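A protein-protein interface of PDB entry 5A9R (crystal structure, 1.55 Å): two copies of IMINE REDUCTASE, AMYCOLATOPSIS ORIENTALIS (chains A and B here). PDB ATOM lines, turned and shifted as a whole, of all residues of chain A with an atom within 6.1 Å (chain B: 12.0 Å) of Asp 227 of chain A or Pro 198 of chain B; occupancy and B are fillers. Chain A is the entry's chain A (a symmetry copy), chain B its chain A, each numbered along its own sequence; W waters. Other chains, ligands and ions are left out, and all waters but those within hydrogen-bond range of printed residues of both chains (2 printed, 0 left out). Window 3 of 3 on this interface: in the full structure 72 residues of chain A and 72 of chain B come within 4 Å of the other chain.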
ATOM      1  N   TYR A 170      18.961 -29.572  33.531  1.00  0.00           N
ATOM      2  CA  TYR A 170      17.616 -30.191  33.496  1.00  0.00           C
ATOM      3  C   TYR A 170      17.085 -30.357  34.883  1.00  0.00           C
ATOM      4  O   TYR A 170      15.929 -30.097  35.167  1.00  0.00           O
ATOM      5  CB  TYR A 170      17.669 -31.577  32.811  1.00  0.00           C
ATOM      6  CG  TYR A 170      17.159 -31.565  31.382  1.00  0.00           C
ATOM      7  CD1 TYR A 170      17.902 -31.095  30.363  1.00  0.00           C
ATOM      8  CD2 TYR A 170      15.912 -32.088  31.152  1.00  0.00           C
ATOM      9  CE1 TYR A 170      17.367 -31.188  29.003  1.00  0.00           C
ATOM     10  CE2 TYR A 170      15.362 -32.117  29.904  1.00  0.00           C
ATOM     11  CZ  TYR A 170      16.109 -31.730  28.858  1.00  0.00           C
ATOM     12  OH  TYR A 170      15.358 -31.774  27.624  1.00  0.00           O
ATOM     13  N   GLU A 222       1.329 -25.526  23.668  1.00  0.00           N
ATOM     14  CA  GLU A 222       1.920 -24.226  23.580  1.00  0.00           C
ATOM     15  C   GLU A 222       3.447 -24.147  23.363  1.00  0.00           C
ATOM     16  O   GLU A 222       4.004 -23.107  22.962  1.00  0.00           O
ATOM     17  CB  GLU A 222       1.565 -23.341  24.771  1.00  0.00           C
ATOM     18  CG  GLU A 222       0.043 -23.146  24.881  1.00  0.00           C
ATOM     19  CD  GLU A 222      -0.551 -22.387  23.682  1.00  0.00           C
ATOM     20  OE1 GLU A 222       0.148 -21.559  23.088  1.00  0.00           O
ATOM     21  OE2 GLU A 222      -1.763 -22.541  23.441  1.00  0.00           O
ATOM     22  N   ALA A 223       4.113 -25.252  23.574  1.00  0.00           N
ATOM     23  CA  ALA A 223       5.573 -25.258  23.512  1.00  0.00           C
ATOM     24  C   ALA A 223       6.122 -24.872  22.112  1.00  0.00           C
ATOM     25  O   ALA A 223       7.013 -24.051  22.017  1.00  0.00           O
ATOM     26  CB  ALA A 223       6.116 -26.550  24.035  1.00  0.00           C
ATOM     27  N   PRO A 224       5.539 -25.360  21.025  1.00  0.00           N
ATOM     28  CA  PRO A 224       6.040 -24.890  19.724  1.00  0.00           C
ATOM     29  C   PRO A 224       5.881 -23.408  19.484  1.00  0.00           C
ATOM     30  O   PRO A 224       6.626 -22.758  18.731  1.00  0.00           O
ATOM     31  CB  PRO A 224       5.232 -25.738  18.746  1.00  0.00           C
ATOM     32  CG  PRO A 224       4.954 -26.978  19.443  1.00  0.00           C
ATOM     33  CD  PRO A 224       4.665 -26.532  20.870  1.00  0.00           C
ATOM     34  N   THR A 225       4.822 -22.813  20.060  1.00  0.00           N
ATOM     35  CA  THR A 225       4.703 -21.358  20.025  1.00  0.00           C
ATOM     36  C   THR A 225       5.839 -20.614  20.706  1.00  0.00           C
ATOM     37  O   THR A 225       6.380 -19.575  20.293  1.00  0.00           O
ATOM     38  CB  THR A 225       3.328 -20.967  20.687  1.00  0.00           C
ATOM     39  OG1 THR A 225       2.282 -21.413  19.823  1.00  0.00           O
ATOM     40  CG2 THR A 225       3.208 -19.565  20.837  1.00  0.00           C
ATOM     41  N   ILE A 226       6.351 -21.134  21.852  1.00  0.00           N
ATOM     42  CA  ILE A 226       7.512 -20.518  22.434  1.00  0.00           C
ATOM     43  C   ILE A 226       8.693 -20.557  21.550  1.00  0.00           C
ATOM     44  O   ILE A 226       9.411 -19.620  21.330  1.00  0.00           O
ATOM     45  CB  ILE A 226       7.892 -21.245  23.804  1.00  0.00           C
ATOM     46  CG1 ILE A 226       6.779 -21.034  24.792  1.00  0.00           C
ATOM     47  CG2 ILE A 226       9.290 -20.848  24.248  1.00  0.00           C
ATOM     48  CD1 ILE A 226       6.825 -21.981  25.995  1.00  0.00           C
ATOM     49  N   ASP A 227       8.913 -21.712  20.920  1.00  0.00           N
ATOM     50  CA  ASP A 227      10.082 -21.824  20.058  1.00  0.00           C
ATOM     51  C   ASP A 227      10.016 -20.935  18.786  1.00  0.00           C
ATOM     52  O   ASP A 227      11.013 -20.431  18.336  1.00  0.00           O
ATOM     53  CB  ASP A 227      10.297 -23.325  19.680  1.00  0.00           C
ATOM     54  CG  ASP A 227      10.546 -24.214  20.860  1.00  0.00           C
ATOM     55  OD1 ASP A 227      11.315 -23.672  21.790  1.00  0.00           O
ATOM     56  OD2 ASP A 227      10.142 -25.451  20.888  1.00  0.00           O
ATOM     57  N   GLU A 228       8.818 -20.702  18.301  1.00  0.00           N
ATOM     58  CA  GLU A 228       8.578 -19.824  17.182  1.00  0.00           C
ATOM     59  C   GLU A 228       8.877 -18.381  17.546  1.00  0.00           C
ATOM     60  O   GLU A 228       9.410 -17.594  16.715  1.00  0.00           O
ATOM     61  CB  GLU A 228       7.135 -19.998  16.687  1.00  0.00           C
ATOM     62  CG  GLU A 228       6.759 -19.037  15.574  1.00  0.00           C
ATOM     63  CD  GLU A 228       5.276 -19.037  15.248  1.00  0.00           C
ATOM     64  OE1 GLU A 228       4.427 -18.944  16.172  1.00  0.00           O
ATOM     65  OE2 GLU A 228       4.913 -19.340  14.074  1.00  0.00           O
ATOM     66  N   GLY A 229       8.489 -18.002  18.781  1.00  0.00           N
ATOM     67  CA  GLY A 229       8.884 -16.685  19.321  1.00  0.00           C
ATOM     68  C   GLY A 229       8.059 -15.439  18.961  1.00  0.00           C
ATOM     69  O   GLY A 229       8.552 -14.300  19.125  1.00  0.00           O
ATOM     70  N   TYR A 231       4.227 -15.338  19.415  1.00  0.00           N
ATOM     71  CA  TYR A 231       3.168 -15.314  20.464  1.00  0.00           C
ATOM     72  C   TYR A 231       1.904 -14.501  20.043  1.00  0.00           C
ATOM     73  O   TYR A 231       1.436 -13.612  20.800  1.00  0.00           O
ATOM     74  CB  TYR A 231       3.753 -14.760  21.744  1.00  0.00           C
ATOM     75  CG  TYR A 231       5.046 -15.377  22.219  1.00  0.00           C
ATOM     76  CD1 TYR A 231       4.970 -16.563  22.907  1.00  0.00           C
ATOM     77  CD2 TYR A 231       6.304 -14.792  22.016  1.00  0.00           C
ATOM     78  CE1 TYR A 231       6.131 -17.138  23.452  1.00  0.00           C
ATOM     79  CE2 TYR A 231       7.484 -15.423  22.512  1.00  0.00           C
ATOM     80  CZ  TYR A 231       7.336 -16.597  23.212  1.00  0.00           C
ATOM     81  OH  TYR A 231       8.490 -17.203  23.691  1.00  0.00           O
ATOM     82  N   ARG A 290      14.819 -14.106  29.632  1.00  0.00           N
ATOM     83  CA  ARG A 290      16.051 -14.501  28.932  1.00  0.00           C
ATOM     84  C   ARG A 290      16.421 -13.506  27.824  1.00  0.00           C
ATOM     85  O   ARG A 290      15.681 -12.545  27.566  1.00  0.00           O
ATOM     86  CB  ARG A 290      15.819 -15.895  28.336  1.00  0.00           C
ATOM     87  CG  ARG A 290      14.507 -16.025  27.515  1.00  0.00           C
ATOM     88  CD  ARG A 290      14.676 -16.597  26.170  1.00  0.00           C
ATOM     89  NE  ARG A 290      13.445 -17.047  25.528  1.00  0.00           N
ATOM     90  CZ  ARG A 290      13.066 -18.333  25.450  1.00  0.00           C
ATOM     91  NH1 ARG A 290      13.785 -19.331  26.042  1.00  0.00           N
ATOM     92  NH2 ARG A 290      11.999 -18.651  24.767  1.00  0.00           N
ATOM     93  N   PHE B 185       6.799 -23.915  34.583  1.00  0.00           N
ATOM     94  CA  PHE B 185       7.281 -24.467  33.347  1.00  0.00           C
ATOM     95  C   PHE B 185       8.056 -23.502  32.476  1.00  0.00           C
ATOM     96  O   PHE B 185       9.104 -23.810  31.881  1.00  0.00           O
ATOM     97  CB  PHE B 185       6.116 -25.068  32.525  1.00  0.00           C
ATOM     98  CG  PHE B 185       6.563 -25.467  31.183  1.00  0.00           C
ATOM     99  CD1 PHE B 185       7.211 -26.691  31.022  1.00  0.00           C
ATOM    100  CD2 PHE B 185       6.417 -24.627  30.100  1.00  0.00           C
ATOM    101  CE1 PHE B 185       7.732 -27.019  29.751  1.00  0.00           C
ATOM    102  CE2 PHE B 185       6.965 -24.950  28.842  1.00  0.00           C
ATOM    103  CZ  PHE B 185       7.572 -26.182  28.657  1.00  0.00           C
ATOM    104  N   LEU B 186       7.574 -22.232  32.424  1.00  0.00           N
ATOM    105  CA  LEU B 186       8.239 -21.224  31.651  1.00  0.00           C
ATOM    106  C   LEU B 186       9.635 -20.856  32.160  1.00  0.00           C
ATOM    107  O   LEU B 186      10.592 -20.708  31.390  1.00  0.00           O
ATOM    108  CB  LEU B 186       7.331 -20.023  31.550  1.00  0.00           C
ATOM    109  CG  LEU B 186       6.038 -20.257  30.738  1.00  0.00           C
ATOM    110  CD1 LEU B 186       5.149 -19.003  30.904  1.00  0.00           C
ATOM    111  CD2 LEU B 186       6.355 -20.503  29.301  1.00  0.00           C
ATOM    112  N   HIS B 187       9.816 -20.866  33.491  1.00  0.00           N
ATOM    113  CA  HIS B 187      11.162 -20.662  34.027  1.00  0.00           C
ATOM    114  C   HIS B 187      12.089 -21.837  33.694  1.00  0.00           C
ATOM    115  O   HIS B 187      13.228 -21.663  33.274  1.00  0.00           O
ATOM    116  CB  HIS B 187      11.098 -20.411  35.552  1.00  0.00           C
ATOM    117  CG  HIS B 187      12.399 -20.062  36.103  1.00  0.00           C
ATOM    118  ND1 HIS B 187      13.151 -20.907  36.860  1.00  0.00           N
ATOM    119  CD2 HIS B 187      13.160 -18.948  35.895  1.00  0.00           C
ATOM    120  CE1 HIS B 187      14.315 -20.336  37.112  1.00  0.00           C
ATOM    121  NE2 HIS B 187      14.362 -19.179  36.504  1.00  0.00           N
ATOM    122  N   ALA B 188      11.518 -23.044  33.790  1.00  0.00           N
ATOM    123  CA  ALA B 188      12.258 -24.261  33.426  1.00  0.00           C
ATOM    124  C   ALA B 188      12.669 -24.227  31.958  1.00  0.00           C
ATOM    125  O   ALA B 188      13.809 -24.517  31.598  1.00  0.00           O
ATOM    126  CB  ALA B 188      11.439 -25.473  33.758  1.00  0.00           C
ATOM    127  N   ALA B 189      11.716 -23.886  31.098  1.00  0.00           N
ATOM    128  CA  ALA B 189      12.024 -23.739  29.701  1.00  0.00           C
ATOM    129  C   ALA B 189      13.038 -22.722  29.365  1.00  0.00           C
ATOM    130  O   ALA B 189      13.870 -22.888  28.461  1.00  0.00           O
ATOM    131  CB  ALA B 189      10.730 -23.545  28.879  1.00  0.00           C
ATOM    132  N   ALA B 190      13.007 -21.560  30.042  1.00  0.00           N
ATOM    133  CA  ALA B 190      14.048 -20.563  29.899  1.00  0.00           C
ATOM    134  C   ALA B 190      15.437 -21.107  30.286  1.00  0.00           C
ATOM    135  O   ALA B 190      16.453 -20.814  29.613  1.00  0.00           O
ATOM    136  CB  ALA B 190      13.715 -19.300  30.655  1.00  0.00           C
ATOM    137  N   LEU B 191      15.450 -21.841  31.395  1.00  0.00           N
ATOM    138  CA  LEU B 191      16.691 -22.451  31.872  1.00  0.00           C
ATOM    139  C   LEU B 191      17.297 -23.448  30.887  1.00  0.00           C
ATOM    140  O   LEU B 191      18.454 -23.278  30.439  1.00  0.00           O
ATOM    141  CB  LEU B 191      16.528 -23.168  33.198  1.00  0.00           C
ATOM    142  CG  LEU B 191      16.508 -22.294  34.408  1.00  0.00           C
ATOM    143  CD1 LEU B 191      15.939 -22.972  35.640  1.00  0.00           C
ATOM    144  CD2 LEU B 191      17.928 -21.754  34.672  1.00  0.00           C
ATOM    145  N   VAL B 192      16.505 -24.404  30.369  1.00  0.00           N
ATOM    146  CA  VAL B 192      17.102 -25.309  29.390  1.00  0.00           C
ATOM    147  C   VAL B 192      17.328 -24.623  28.059  1.00  0.00           C
ATOM    148  O   VAL B 192      18.244 -24.971  27.291  1.00  0.00           O
ATOM    149  CB  VAL B 192      16.357 -26.616  29.242  1.00  0.00           C
ATOM    150  CG1 VAL B 192      16.322 -27.416  30.528  1.00  0.00           C
ATOM    151  CG2 VAL B 192      14.937 -26.472  28.706  1.00  0.00           C
ATOM    152  N   GLY B 193      16.531 -23.608  27.787  1.00  0.00           N
ATOM    153  CA  GLY B 193      16.680 -22.811  26.564  1.00  0.00           C
ATOM    154  C   GLY B 193      17.982 -22.025  26.466  1.00  0.00           C
ATOM    155  O   GLY B 193      18.535 -21.817  25.375  1.00  0.00           O
ATOM    156  N   SER B 194      18.570 -21.715  27.614  1.00  0.00           N
ATOM    157  CA  SER B 194      19.845 -21.037  27.669  1.00  0.00           C
ATOM    158  C   SER B 194      20.957 -21.964  27.233  1.00  0.00           C
ATOM    159  O   SER B 194      22.026 -21.458  26.920  1.00  0.00           O
ATOM    160  CB  SER B 194      20.082 -20.476  29.084  1.00  0.00           C
ATOM    161  OG  SER B 194      20.426 -21.502  29.994  1.00  0.00           O
ATOM    162  N   ALA B 195      20.740 -23.282  27.085  1.00  0.00           N
ATOM    163  CA  ALA B 195      21.684 -24.211  26.544  1.00  0.00           C
ATOM    164  C   ALA B 195      21.265 -24.740  25.176  1.00  0.00           C
ATOM    165  O   ALA B 195      21.832 -25.718  24.674  1.00  0.00           O
ATOM    166  CB  ALA B 195      21.923 -25.317  27.503  1.00  0.00           C
ATOM    167  N   GLY B 196      20.266 -24.087  24.601  1.00  0.00           N
ATOM    168  CA  GLY B 196      19.804 -24.386  23.301  1.00  0.00           C
ATOM    169  C   GLY B 196      18.734 -25.423  23.194  1.00  0.00           C
ATOM    170  O   GLY B 196      18.428 -25.811  22.057  1.00  0.00           O
ATOM    171  N   VAL B 197      18.095 -25.875  24.284  1.00  0.00           N
ATOM    172  CA  VAL B 197      17.121 -26.945  24.216  1.00  0.00           C
ATOM    173  C   VAL B 197      15.779 -26.286  23.891  1.00  0.00           C
ATOM    174  O   VAL B 197      15.296 -25.470  24.674  1.00  0.00           O
ATOM    175  CB  VAL B 197      16.943 -27.680  25.585  1.00  0.00           C
ATOM    176  CG1 VAL B 197      15.848 -28.701  25.515  1.00  0.00           C
ATOM    177  CG2 VAL B 197      18.253 -28.347  26.019  1.00  0.00           C
ATOM    178  N   PRO B 198      15.119 -26.645  22.779  1.00  0.00           N
ATOM    179  CA  PRO B 198      13.789 -26.133  22.482  1.00  0.00           C
ATOM    180  C   PRO B 198      12.765 -26.539  23.507  1.00  0.00           C
ATOM    181  O   PRO B 198      12.793 -27.615  24.103  1.00  0.00           O
ATOM    182  CB  PRO B 198      13.422 -26.767  21.112  1.00  0.00           C
ATOM    183  CG  PRO B 198      14.731 -27.308  20.592  1.00  0.00           C
ATOM    184  CD  PRO B 198      15.580 -27.666  21.791  1.00  0.00           C
ATOM    185  N   ALA B 199      11.820 -25.642  23.717  1.00  0.00           N
ATOM    186  CA  ALA B 199      10.760 -25.912  24.643  1.00  0.00           C
ATOM    187  C   ALA B 199       9.946 -27.174  24.310  1.00  0.00           C
ATOM    188  O   ALA B 199       9.548 -27.969  25.130  1.00  0.00           O
ATOM    189  CB  ALA B 199       9.861 -24.672  24.782  1.00  0.00           C
ATOM    190  N   ALA B 200       9.693 -27.355  22.989  1.00  0.00           N
ATOM    191  CA  ALA B 200       8.931 -28.532  22.607  1.00  0.00           C
ATOM    192  C   ALA B 200       9.679 -29.821  22.880  1.00  0.00           C
ATOM    193  O   ALA B 200       9.078 -30.788  23.285  1.00  0.00           O
ATOM    194  CB  ALA B 200       8.534 -28.412  21.133  1.00  0.00           C
ATOM    195  N   GLU B 201      11.029 -29.821  22.750  1.00  0.00           N
ATOM    196  CA  GLU B 201      11.836 -30.944  23.159  1.00  0.00           C
ATOM    197  C   GLU B 201      11.771 -31.238  24.656  1.00  0.00           C
ATOM    198  O   GLU B 201      11.626 -32.341  25.136  1.00  0.00           O
ATOM    199  CB  GLU B 201      13.282 -30.766  22.637  1.00  0.00           C
ATOM    200  CG  GLU B 201      14.303 -31.829  23.061  1.00  0.00           C
ATOM    201  CD  GLU B 201      14.013 -33.200  22.426  1.00  0.00           C
ATOM    202  OE1 GLU B 201      13.193 -33.292  21.467  1.00  0.00           O
ATOM    203  OE2 GLU B 201      14.599 -34.228  22.895  1.00  0.00           O
ATOM    204  N   PHE B 202      11.870 -30.148  25.397  1.00  0.00           N
ATOM    205  CA  PHE B 202      11.861 -30.210  26.848  1.00  0.00           C
ATOM    206  C   PHE B 202      10.563 -30.817  27.366  1.00  0.00           C
ATOM    207  O   PHE B 202      10.603 -31.567  28.314  1.00  0.00           O
ATOM    208  CB  PHE B 202      12.077 -28.779  27.436  1.00  0.00           C
ATOM    209  CG  PHE B 202      12.118 -28.677  28.944  1.00  0.00           C
ATOM    210  CD1 PHE B 202      12.976 -29.453  29.710  1.00  0.00           C
ATOM    211  CD2 PHE B 202      11.245 -27.862  29.572  1.00  0.00           C
ATOM    212  CE1 PHE B 202      12.978 -29.360  31.073  1.00  0.00           C
ATOM    213  CE2 PHE B 202      11.184 -27.773  30.959  1.00  0.00           C
ATOM    214  CZ  PHE B 202      12.121 -28.489  31.672  1.00  0.00           C
ATOM    215  N   THR B 203       9.439 -30.580  26.685  1.00  0.00           N
ATOM    216  CA  THR B 203       8.209 -31.166  27.183  1.00  0.00           C
ATOM    217  C   THR B 203       8.155 -32.692  27.228  1.00  0.00           C
ATOM    218  O   THR B 203       7.403 -33.267  27.981  1.00  0.00           O
ATOM    219  CB  THR B 203       6.972 -30.680  26.399  1.00  0.00           C
ATOM    220  OG1 THR B 203       7.030 -31.199  25.065  1.00  0.00           O
ATOM    221  CG2 THR B 203       6.844 -29.175  26.335  1.00  0.00           C
ATOM    222  N   LYS B 204       9.000 -33.356  26.440  1.00  0.00           N
ATOM    223  CA  LYS B 204       9.041 -34.793  26.481  1.00  0.00           C
ATOM    224  C   LYS B 204       9.382 -35.328  27.866  1.00  0.00           C
ATOM    225  O   LYS B 204       8.648 -36.136  28.397  1.00  0.00           O
ATOM    226  CB  LYS B 204      10.008 -35.332  25.448  1.00  0.00           C
ATOM    227  CG  LYS B 204       9.645 -34.970  24.010  1.00  0.00           C
ATOM    228  CD  LYS B 204      10.724 -35.472  23.073  1.00  0.00           C
ATOM    229  CE  LYS B 204      10.427 -35.034  21.667  1.00  0.00           C
ATOM    230  NZ  LYS B 204      11.662 -35.342  20.895  1.00  0.00           N
ATOM    231  N   LEU B 205      10.395 -34.766  28.516  1.00  0.00           N
ATOM    232  CA  LEU B 205      10.669 -35.139  29.882  1.00  0.00           C
ATOM    233  C   LEU B 205       9.813 -34.374  30.903  1.00  0.00           C
ATOM    234  O   LEU B 205       9.358 -34.951  31.860  1.00  0.00           O
ATOM    235  CB  LEU B 205      12.150 -34.899  30.160  1.00  0.00           C
ATOM    236  CG  LEU B 205      13.045 -36.007  29.607  1.00  0.00           C
ATOM    237  CD1 LEU B 205      14.520 -35.598  29.854  1.00  0.00           C
ATOM    238  CD2 LEU B 205      12.739 -37.310  30.333  1.00  0.00           C
ATOM    239  N   ALA B 206       9.576 -33.098  30.638  1.00  0.00           N
ATOM    240  CA  ALA B 206       8.931 -32.282  31.650  1.00  0.00           C
ATOM    241  C   ALA B 206       7.462 -32.555  31.843  1.00  0.00           C
ATOM    242  O   ALA B 206       6.947 -32.564  32.947  1.00  0.00           O
ATOM    243  CB  ALA B 206       9.145 -30.873  31.344  1.00  0.00           C
ATOM    244  N   VAL B 207       6.768 -32.796  30.736  1.00  0.00           N
ATOM    245  CA  VAL B 207       5.319 -33.045  30.780  1.00  0.00           C
ATOM    246  C   VAL B 207       4.941 -34.510  30.672  1.00  0.00           C
ATOM    247  O   VAL B 207       4.100 -35.020  31.454  1.00  0.00           O
ATOM    248  CB  VAL B 207       4.588 -32.250  29.666  1.00  0.00           C
ATOM    249  CG1 VAL B 207       3.095 -32.676  29.696  1.00  0.00           C
ATOM    250  CG2 VAL B 207       4.797 -30.787  29.791  1.00  0.00           C
ATOM    251  N   ASP B 208       5.610 -35.249  29.759  1.00  0.00           N
ATOM    252  CA  ASP B 208       5.183 -36.650  29.632  1.00  0.00           C
ATOM    253  C   ASP B 208       5.617 -37.517  30.787  1.00  0.00           C
ATOM    254  O   ASP B 208       4.987 -38.512  31.102  1.00  0.00           O
ATOM    255  CB  ASP B 208       5.709 -37.260  28.328  1.00  0.00           C
ATOM    256  CG  ASP B 208       5.259 -36.565  27.127  1.00  0.00           C
ATOM    257  OD1 ASP B 208       4.210 -35.945  27.151  1.00  0.00           O
ATOM    258  OD2 ASP B 208       5.939 -36.691  26.110  1.00  0.00           O
HETATM  259  O   HOH W   1      16.370 -19.154  27.552  1.00  0.00           O
HETATM  260  O   HOH W   2      13.117 -33.676  27.080  1.00  0.00           O
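OD1 of Asp 227 of chain A lies within hydrogen-bond range of N of Ala 199 of chain B, at 2.8 Å. The backbone NH (N) of Ala 200 of chain B is in hydrogen-bond range of the side-chain carboxylate (OD2) of Asp 227 of chain A (2.9 Å).
The backbone NH (N) of Asp 208 of chain B sits at hydrogen-bond distance from the backbone carbonyl oxygen (O) of Thr 203 of chain B (3.2 Å). The backbone NH of Val 197 of chain B is in hydrogen-bond range of the backbone carbonyl oxygen of Val 192 of chain B, at 3.1 Å. OG1 of Thr 203 of chain B lies within hydrogen-bond range of O of Ala 200 of chain B (2.7 Å).
CG1 of Val 197 of chain B touches OH of Tyr 170 of chain A, 3.8 Å away. Tyr 170 of chain A touches Phe 202 of chain B. Tyr 170 of chain A touches Leu 205 of chain B (CE2 to CD1, 3.6 Å). Ala 223 of chain A touches Ala 199 of chain B (CB to O, 3.9 Å). Ala 223 of chain A touches Ala 200 of chain B (CB to CA, 3.7 Å). Thr 203 of chain B touches Ala 223 of chain A (CG2 to CB, 3.6 Å). CD2 of Leu 186 of chain B touches CD1 of Ile 226 of chain A (3.7 Å). Ala 199 of chain B touches Ile 226 of chain A. CB of Pro 198 of chain B touches OD2 of Asp 227 of chain A (3.5 Å).
Printed residues of chain B within 4 Å of Tyr 170 of chain A: Val 197 (3.8 Å), Phe 202 (3.6 Å) and Leu 205 (3.6 Å). Ala 223 of chain A touches just these residues of chain B: Ala 199, Ala 200 and Thr 203. No residue of chain B comes within 4 Å of Pro 224 of chain A. Of chain B, only Pro 198 (3.5 Å), Ala 199 (2.8 Å) and Ala 200 (2.9 Å) come within 4 Å of Asp 227 of chain A. No residue of chain B comes within 4 Å of Glu 228 of chain A. No residue of chain B comes within 4 Å of Gly 229 of chain A. Of the printed residues of chain A, Pro 198 of chain B touches Asp 227 (3.5 Å). Printed residues of chain A within 4 Å of Ala 199 of chain B: Ala 223 (3.9 Å), Ile 226 (3.9 Å) and Asp 227 (2.8 Å). Of the printed residues of chain A, Ala 200 of chain B touches Ala 223 and Asp 227. Printed residues of chain A within 4 Å of Phe 202 of chain B: Tyr 170 (3.6 Å). The nearest residue of chain B that does not touch Asp 227 of chain A is Glu 201 of chain B (4.8 Å). The nearest residue of chain A that does not touch Pro 198 of chain B is Tyr 170 of chain A (6.0 Å).
Of the 11 printed residues of chain A, 4 touch a printed residue of chain B. Hydrophobic or aromatic side chains of chain A that line the printed part of chain B: Tyr 170, Ala 223 and Ile 226. Among the printed residues, 11 pairs touch across the chains. Among the printed residues, no Asp or Glu carboxylate lies within 4 Å of a Lys or Arg side-chain nitrogen of the other chain.
No position is printed for both chains. Of the 11 pairs that touch across the chains among the printed residues, none has its exchanged pair printed and touching as well.
Water W1 lies within hydrogen-bond range of O of Ala 190 of chain B, NH1 of Arg 290 of chain A and N of Ser 194 of chain B. Water W2 lies within hydrogen-bond range of O of Glu 201 of chain B, OH of Tyr 170 of chain A and N of Leu 205 of chain B.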
